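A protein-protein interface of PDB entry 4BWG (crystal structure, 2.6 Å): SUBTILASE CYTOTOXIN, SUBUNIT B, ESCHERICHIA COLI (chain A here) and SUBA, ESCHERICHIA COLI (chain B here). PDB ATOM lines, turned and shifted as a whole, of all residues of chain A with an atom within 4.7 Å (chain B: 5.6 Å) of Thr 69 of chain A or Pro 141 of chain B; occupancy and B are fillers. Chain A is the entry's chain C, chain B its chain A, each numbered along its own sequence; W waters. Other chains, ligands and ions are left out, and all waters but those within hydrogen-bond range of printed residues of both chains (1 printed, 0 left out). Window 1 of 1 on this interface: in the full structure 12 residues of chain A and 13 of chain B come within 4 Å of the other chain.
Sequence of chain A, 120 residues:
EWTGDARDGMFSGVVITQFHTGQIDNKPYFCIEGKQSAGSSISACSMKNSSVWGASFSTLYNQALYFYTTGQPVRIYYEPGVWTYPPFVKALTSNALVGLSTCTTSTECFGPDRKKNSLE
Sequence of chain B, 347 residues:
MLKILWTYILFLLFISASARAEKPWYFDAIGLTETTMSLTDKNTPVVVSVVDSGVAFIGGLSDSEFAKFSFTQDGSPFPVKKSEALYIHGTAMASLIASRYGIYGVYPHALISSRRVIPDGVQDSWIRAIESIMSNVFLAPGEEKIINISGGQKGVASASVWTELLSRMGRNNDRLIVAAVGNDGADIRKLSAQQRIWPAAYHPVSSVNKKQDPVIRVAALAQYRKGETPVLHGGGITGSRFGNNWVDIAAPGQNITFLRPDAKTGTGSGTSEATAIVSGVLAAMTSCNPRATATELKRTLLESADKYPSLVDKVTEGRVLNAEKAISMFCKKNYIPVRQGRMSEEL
NE of Arg 291 of chain B is in hydrogen-bond range of O of Tyr 68 of chain A (2.6 Å).
O of Pro 290 of chain B is in hydrogen-bond range of NZ of Lys 145 of chain B (3.1 Å).
OG1 of Thr 70 of chain A is in hydrogen-bond range of O of Phe 67 of chain A (3.4 Å).
The side-chain hydroxyl (OG1) of Thr 69 of chain A sits at hydrogen-bond distance from the backbone carbonyl oxygen (O) of Leu 65 of chain A (2.8 Å).
The backbone NH of Arg 291 of chain B sits close to the side-chain amide oxygen of Asn 289 of chain B (3.1 Å).
O of Thr 69 of chain A touches CG of Pro 141 of chain B, at 3.9 Å.
OD1 of Asn 289 of chain B touches CG2 of Thr 69 of chain A (3.2 Å).
Thr 69 of chain A touches Pro 290 of chain B (O to CG, 2.9 Å).
Thr 69 of chain A touches Arg 291 of chain B (O to CG, 3.8 Å).
Thr 69 of chain A touches Val 338 of chain B (CG2 to CG2, 3.8 Å).
Thr 70 of chain A touches Thr 44 of chain B.
Pro 45 of chain B touches Thr 70 of chain A (CD to O, 3.2 Å).
Pro 290 of chain B touches Thr 70 of chain A (CG to O, 3.9 Å).
Ala 140 of chain B touches Gly 71 of chain A (CB to O, 3.3 Å).
CA of Gly 71 of chain A touches CD of Pro 141 of chain B, at 3.6 Å.
Pro 141 of chain B touches two residues of chain A.
Of the printed residues of chain A, Thr 44 of chain B touches Thr 70.
Printed residues of chain A within 4 Å of Arg 291 of chain B: Tyr 68 (2.6 Å) and Thr 69 (3.8 Å).
Printed residues of chain B within 4 Å of Tyr 68 of chain A: Arg 291 (2.6 Å).
The nearest residue of chain B that does not touch Thr 69 of chain A is Cys 288 of chain B (4.6 Å).
Hydrophobic or aromatic side chains of chain B within 4 Å of the printed part of chain A: Pro 45, Ala 140, Pro 141, Pro 290 and Val 338.
Along chain B the printed residues that touch a printed residue of chain A span positions 44 to 338.
Among the printed residues, 12 pairs touch across the chains.
Water W1 lies within hydrogen-bond range of O of Pro 45 of chain B (2.8 Å), O of Thr 70 of chain A (2.8 Å) and N of Gly 142 of chain B (2.8 Å).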
ATOM      1  N   LEU A  65     -19.700 -28.825 -31.781  1.00  0.00           N
ATOM      2  CA  LEU A  65     -20.831 -27.961 -31.460  1.00  0.00           C
ATOM      3  C   LEU A  65     -21.164 -28.047 -29.971  1.00  0.00           C
ATOM      4  O   LEU A  65     -21.471 -27.016 -29.352  1.00  0.00           O
ATOM      5  CB  LEU A  65     -22.055 -28.261 -32.333  1.00  0.00           C
ATOM      6  CG  LEU A  65     -23.280 -27.327 -32.113  1.00  0.00           C
ATOM      7  CD1 LEU A  65     -22.930 -25.876 -32.394  1.00  0.00           C
ATOM      8  CD2 LEU A  65     -24.455 -27.768 -32.954  1.00  0.00           C
ATOM      9  N   TYR A  66     -21.058 -29.258 -29.396  1.00  0.00           N
ATOM     10  CA  TYR A  66     -21.258 -29.474 -27.968  1.00  0.00           C
ATOM     11  C   TYR A  66     -20.238 -28.656 -27.144  1.00  0.00           C
ATOM     12  O   TYR A  66     -20.615 -27.935 -26.220  1.00  0.00           O
ATOM     13  CB  TYR A  66     -21.169 -30.976 -27.603  1.00  0.00           C
ATOM     14  CG  TYR A  66     -21.403 -31.179 -26.122  1.00  0.00           C
ATOM     15  CD1 TYR A  66     -22.691 -31.035 -25.567  1.00  0.00           C
ATOM     16  CD2 TYR A  66     -20.332 -31.364 -25.247  1.00  0.00           C
ATOM     17  CE1 TYR A  66     -22.899 -31.076 -24.185  1.00  0.00           C
ATOM     18  CE2 TYR A  66     -20.543 -31.482 -23.866  1.00  0.00           C
ATOM     19  CZ  TYR A  66     -21.836 -31.351 -23.344  1.00  0.00           C
ATOM     20  OH  TYR A  66     -22.073 -31.302 -21.996  1.00  0.00           O
ATOM     21  N   PHE A  67     -18.965 -28.771 -27.458  1.00  0.00           N
ATOM     22  CA  PHE A  67     -17.907 -28.077 -26.723  1.00  0.00           C
ATOM     23  C   PHE A  67     -17.961 -26.561 -26.927  1.00  0.00           C
ATOM     24  O   PHE A  67     -17.587 -25.811 -26.007  1.00  0.00           O
ATOM     25  CB  PHE A  67     -16.560 -28.621 -27.152  1.00  0.00           C
ATOM     26  CG  PHE A  67     -16.253 -29.998 -26.626  1.00  0.00           C
ATOM     27  CD1 PHE A  67     -16.746 -30.426 -25.380  1.00  0.00           C
ATOM     28  CD2 PHE A  67     -15.377 -30.834 -27.306  1.00  0.00           C
ATOM     29  CE1 PHE A  67     -16.383 -31.688 -24.858  1.00  0.00           C
ATOM     30  CE2 PHE A  67     -15.016 -32.087 -26.778  1.00  0.00           C
ATOM     31  CZ  PHE A  67     -15.514 -32.504 -25.561  1.00  0.00           C
ATOM     32  N   TYR A  68     -18.436 -26.104 -28.122  1.00  0.00           N
ATOM     33  CA  TYR A  68     -18.688 -24.688 -28.376  1.00  0.00           C
ATOM     34  C   TYR A  68     -19.735 -24.206 -27.409  1.00  0.00           C
ATOM     35  O   TYR A  68     -19.592 -23.106 -26.885  1.00  0.00           O
ATOM     36  CB  TYR A  68     -19.141 -24.417 -29.839  1.00  0.00           C
ATOM     37  CG  TYR A  68     -19.653 -23.005 -30.065  1.00  0.00           C
ATOM     38  CD1 TYR A  68     -18.786 -21.926 -30.086  1.00  0.00           C
ATOM     39  CD2 TYR A  68     -21.017 -22.744 -30.201  1.00  0.00           C
ATOM     40  CE1 TYR A  68     -19.257 -20.624 -30.246  1.00  0.00           C
ATOM     41  CE2 TYR A  68     -21.491 -21.447 -30.387  1.00  0.00           C
ATOM     42  CZ  TYR A  68     -20.610 -20.391 -30.384  1.00  0.00           C
ATOM     43  OH  TYR A  68     -21.067 -19.102 -30.465  1.00  0.00           O
ATOM     44  N   THR A  69     -20.800 -25.021 -27.188  1.00  0.00           N
ATOM     45  CA  THR A  69     -21.910 -24.685 -26.302  1.00  0.00           C
ATOM     46  C   THR A  69     -21.444 -24.567 -24.847  1.00  0.00           C
ATOM     47  O   THR A  69     -21.742 -23.552 -24.213  1.00  0.00           O
ATOM     48  CB  THR A  69     -23.052 -25.691 -26.448  1.00  0.00           C
ATOM     49  OG1 THR A  69     -23.421 -25.775 -27.829  1.00  0.00           O
ATOM     50  CG2 THR A  69     -24.245 -25.334 -25.607  1.00  0.00           C
ATOM     51  N   THR A  70     -20.720 -25.583 -24.322  1.00  0.00           N
ATOM     52  CA  THR A  70     -20.316 -25.567 -22.919  1.00  0.00           C
ATOM     53  C   THR A  70     -19.244 -24.494 -22.628  1.00  0.00           C
ATOM     54  O   THR A  70     -19.210 -23.904 -21.542  1.00  0.00           O
ATOM     55  CB  THR A  70     -19.836 -26.957 -22.450  1.00  0.00           C
ATOM     56  OG1 THR A  70     -18.620 -27.293 -23.095  1.00  0.00           O
ATOM     57  CG2 THR A  70     -20.867 -28.028 -22.635  1.00  0.00           C
ATOM     58  N   GLY A  71     -18.362 -24.273 -23.587  1.00  0.00           N
ATOM     59  CA  GLY A  71     -17.248 -23.363 -23.375  1.00  0.00           C
ATOM     60  C   GLY A  71     -16.157 -23.977 -22.500  1.00  0.00           C
ATOM     61  O   GLY A  71     -15.222 -23.287 -22.112  1.00  0.00           O
ATOM     62  N   THR B  44     -20.552 -27.691 -18.204  1.00  0.00           N
ATOM     63  CA  THR B  44     -20.483 -26.273 -18.473  1.00  0.00           C
ATOM     64  C   THR B  44     -19.802 -25.492 -17.352  1.00  0.00           C
ATOM     65  O   THR B  44     -20.386 -25.369 -16.271  1.00  0.00           O
ATOM     66  CB  THR B  44     -21.883 -25.694 -18.737  1.00  0.00           C
ATOM     67  OG1 THR B  44     -22.548 -26.500 -19.687  1.00  0.00           O
ATOM     68  CG2 THR B  44     -21.826 -24.294 -19.299  1.00  0.00           C
ATOM     69  N   PRO B  45     -18.649 -24.823 -17.630  1.00  0.00           N
ATOM     70  CA  PRO B  45     -18.065 -23.923 -16.619  1.00  0.00           C
ATOM     71  C   PRO B  45     -18.996 -22.735 -16.351  1.00  0.00           C
ATOM     72  O   PRO B  45     -19.277 -21.923 -17.230  1.00  0.00           O
ATOM     73  CB  PRO B  45     -16.744 -23.481 -17.277  1.00  0.00           C
ATOM     74  CG  PRO B  45     -16.502 -24.433 -18.358  1.00  0.00           C
ATOM     75  CD  PRO B  45     -17.832 -24.827 -18.861  1.00  0.00           C
ATOM     76  N   LEU B 139     -12.781 -16.541 -21.488  1.00  0.00           N
ATOM     77  CA  LEU B 139     -13.373 -16.901 -22.785  1.00  0.00           C
ATOM     78  C   LEU B 139     -14.668 -17.692 -22.717  1.00  0.00           C
ATOM     79  O   LEU B 139     -15.486 -17.515 -23.620  1.00  0.00           O
ATOM     80  CB  LEU B 139     -12.379 -17.684 -23.651  1.00  0.00           C
ATOM     81  CG  LEU B 139     -11.048 -17.004 -23.913  1.00  0.00           C
ATOM     82  CD1 LEU B 139      -9.973 -18.024 -24.208  1.00  0.00           C
ATOM     83  CD2 LEU B 139     -11.179 -15.941 -24.944  1.00  0.00           C
ATOM     84  N   ALA B 140     -14.844 -18.589 -21.717  1.00  0.00           N
ATOM     85  CA  ALA B 140     -16.023 -19.437 -21.648  1.00  0.00           C
ATOM     86  C   ALA B 140     -17.297 -18.598 -21.529  1.00  0.00           C
ATOM     87  O   ALA B 140     -17.335 -17.656 -20.737  1.00  0.00           O
ATOM     88  CB  ALA B 140     -15.922 -20.439 -20.507  1.00  0.00           C
ATOM     89  N   PRO B 141     -18.345 -18.913 -22.346  1.00  0.00           N
ATOM     90  CA  PRO B 141     -19.593 -18.129 -22.292  1.00  0.00           C
ATOM     91  C   PRO B 141     -20.241 -18.021 -20.881  1.00  0.00           C
ATOM     92  O   PRO B 141     -20.818 -16.995 -20.585  1.00  0.00           O
ATOM     93  CB  PRO B 141     -20.501 -18.867 -23.290  1.00  0.00           C
ATOM     94  CG  PRO B 141     -19.892 -20.216 -23.482  1.00  0.00           C
ATOM     95  CD  PRO B 141     -18.444 -19.991 -23.362  1.00  0.00           C
ATOM     96  N   GLY B 142     -20.135 -19.054 -20.033  1.00  0.00           N
ATOM     97  CA  GLY B 142     -20.727 -19.062 -18.689  1.00  0.00           C
ATOM     98  C   GLY B 142     -19.899 -18.502 -17.543  1.00  0.00           C
ATOM     99  O   GLY B 142     -20.280 -18.616 -16.379  1.00  0.00           O
ATOM    100  N   GLU B 143     -18.768 -17.892 -17.853  1.00  0.00           N
ATOM    101  CA  GLU B 143     -17.909 -17.282 -16.852  1.00  0.00           C
ATOM    102  C   GLU B 143     -18.278 -15.812 -16.746  1.00  0.00           C
ATOM    103  O   GLU B 143     -18.062 -15.060 -17.699  1.00  0.00           O
ATOM    104  CB  GLU B 143     -16.421 -17.512 -17.183  1.00  0.00           C
ATOM    105  CG  GLU B 143     -16.078 -18.992 -17.044  1.00  0.00           C
ATOM    106  CD  GLU B 143     -14.697 -19.441 -17.477  1.00  0.00           C
ATOM    107  OE1 GLU B 143     -14.038 -18.722 -18.259  1.00  0.00           O
ATOM    108  OE2 GLU B 143     -14.306 -20.562 -17.084  1.00  0.00           O
ATOM    109  N   GLU B 144     -18.957 -15.451 -15.628  1.00  0.00           N
ATOM    110  CA  GLU B 144     -19.438 -14.106 -15.290  1.00  0.00           C
ATOM    111  C   GLU B 144     -20.520 -13.607 -16.267  1.00  0.00           C
ATOM    112  O   GLU B 144     -20.599 -12.400 -16.566  1.00  0.00           O
ATOM    113  CB  GLU B 144     -18.303 -13.086 -15.181  1.00  0.00           C
ATOM    114  CG  GLU B 144     -17.348 -13.322 -14.027  1.00  0.00           C
ATOM    115  CD  GLU B 144     -16.286 -12.237 -13.890  1.00  0.00           C
ATOM    116  OE1 GLU B 144     -15.643 -11.886 -14.912  1.00  0.00           O
ATOM    117  OE2 GLU B 144     -16.087 -11.745 -12.755  1.00  0.00           O
ATOM    118  N   LYS B 145     -21.376 -14.550 -16.732  1.00  0.00           N
ATOM    119  CA  LYS B 145     -22.534 -14.276 -17.568  1.00  0.00           C
ATOM    120  C   LYS B 145     -23.616 -13.717 -16.661  1.00  0.00           C
ATOM    121  O   LYS B 145     -24.415 -12.886 -17.084  1.00  0.00           O
ATOM    122  CB  LYS B 145     -22.996 -15.568 -18.253  1.00  0.00           C
ATOM    123  CG  LYS B 145     -24.043 -15.364 -19.324  1.00  0.00           C
ATOM    124  CD  LYS B 145     -24.387 -16.635 -20.039  1.00  0.00           C
ATOM    125  CE  LYS B 145     -25.490 -16.368 -21.059  1.00  0.00           C
ATOM    126  NZ  LYS B 145     -24.997 -15.661 -22.263  1.00  0.00           N
ATOM    127  N   ARG B 175     -24.601 -10.740 -21.019  1.00  0.00           N
ATOM    128  CA  ARG B 175     -24.616 -10.800 -19.548  1.00  0.00           C
ATOM    129  C   ARG B 175     -25.887 -10.216 -18.942  1.00  0.00           C
ATOM    130  O   ARG B 175     -26.545  -9.350 -19.531  1.00  0.00           O
ATOM    131  CB  ARG B 175     -23.400 -10.073 -18.941  1.00  0.00           C
ATOM    132  CG  ARG B 175     -22.081 -10.484 -19.578  1.00  0.00           C
ATOM    133  CD  ARG B 175     -20.881  -9.818 -18.952  1.00  0.00           C
ATOM    134  NE  ARG B 175     -19.709  -9.947 -19.806  1.00  0.00           N
ATOM    135  CZ  ARG B 175     -18.892 -10.996 -19.843  1.00  0.00           C
ATOM    136  NH1 ARG B 175     -19.080 -12.021 -19.022  1.00  0.00           N
ATOM    137  NH2 ARG B 175     -17.876 -11.023 -20.696  1.00  0.00           N
ATOM    138  N   CYS B 288     -27.229 -25.191 -19.007  1.00  0.00           N
ATOM    139  CA  CYS B 288     -27.884 -25.886 -20.101  1.00  0.00           C
ATOM    140  C   CYS B 288     -27.513 -25.330 -21.502  1.00  0.00           C
ATOM    141  O   CYS B 288     -27.609 -26.050 -22.487  1.00  0.00           O
ATOM    142  CB  CYS B 288     -29.396 -25.913 -19.864  1.00  0.00           C
ATOM    143  SG  CYS B 288     -29.893 -27.262 -18.758  1.00  0.00           S
ATOM    144  N   ASN B 289     -27.108 -24.071 -21.592  1.00  0.00           N
ATOM    145  CA  ASN B 289     -26.660 -23.392 -22.827  1.00  0.00           C
ATOM    146  C   ASN B 289     -26.191 -21.988 -22.484  1.00  0.00           C
ATOM    147  O   ASN B 289     -26.982 -21.053 -22.529  1.00  0.00           O
ATOM    148  CB  ASN B 289     -27.723 -23.346 -23.943  1.00  0.00           C
ATOM    149  CG  ASN B 289     -27.152 -23.066 -25.310  1.00  0.00           C
ATOM    150  OD1 ASN B 289     -26.008 -22.642 -25.454  1.00  0.00           O
ATOM    151  ND2 ASN B 289     -27.905 -23.373 -26.359  1.00  0.00           N
ATOM    152  N   PRO B 290     -24.891 -21.815 -22.150  1.00  0.00           N
ATOM    153  CA  PRO B 290     -24.377 -20.466 -21.854  1.00  0.00           C
ATOM    154  C   PRO B 290     -24.223 -19.597 -23.115  1.00  0.00           C
ATOM    155  O   PRO B 290     -23.870 -18.442 -23.009  1.00  0.00           O
ATOM    156  CB  PRO B 290     -23.026 -20.766 -21.213  1.00  0.00           C
ATOM    157  CG  PRO B 290     -22.588 -22.020 -21.858  1.00  0.00           C
ATOM    158  CD  PRO B 290     -23.808 -22.827 -22.075  1.00  0.00           C
ATOM    159  N   ARG B 291     -24.516 -20.138 -24.301  1.00  0.00           N
ATOM    160  CA  ARG B 291     -24.429 -19.390 -25.561  1.00  0.00           C
ATOM    161  C   ARG B 291     -25.710 -18.627 -25.819  1.00  0.00           C
ATOM    162  O   ARG B 291     -25.732 -17.742 -26.676  1.00  0.00           O
ATOM    163  CB  ARG B 291     -24.113 -20.303 -26.741  1.00  0.00           C
ATOM    164  CG  ARG B 291     -22.736 -20.899 -26.673  1.00  0.00           C
ATOM    165  CD  ARG B 291     -21.658 -19.884 -26.998  1.00  0.00           C
ATOM    166  NE  ARG B 291     -20.400 -20.604 -27.014  1.00  0.00           N
ATOM    167  CZ  ARG B 291     -19.196 -20.065 -27.013  1.00  0.00           C
ATOM    168  NH1 ARG B 291     -19.050 -18.743 -27.069  1.00  0.00           N
ATOM    169  NH2 ARG B 291     -18.126 -20.840 -26.987  1.00  0.00           N
ATOM    170  N   VAL B 338     -28.580 -28.930 -27.995  1.00  0.00           N
ATOM    171  CA  VAL B 338     -27.403 -29.203 -27.168  1.00  0.00           C
ATOM    172  C   VAL B 338     -27.192 -30.687 -26.797  1.00  0.00           C
ATOM    173  O   VAL B 338     -26.047 -31.131 -26.844  1.00  0.00           O
ATOM    174  CB  VAL B 338     -27.444 -28.347 -25.882  1.00  0.00           C
ATOM    175  CG1 VAL B 338     -26.197 -28.560 -25.028  1.00  0.00           C
ATOM    176  CG2 VAL B 338     -27.612 -26.870 -26.222  1.00  0.00           C
HETATM  177  O   HOH W   1     -19.087 -21.634 -19.972  1.00  0.00           O
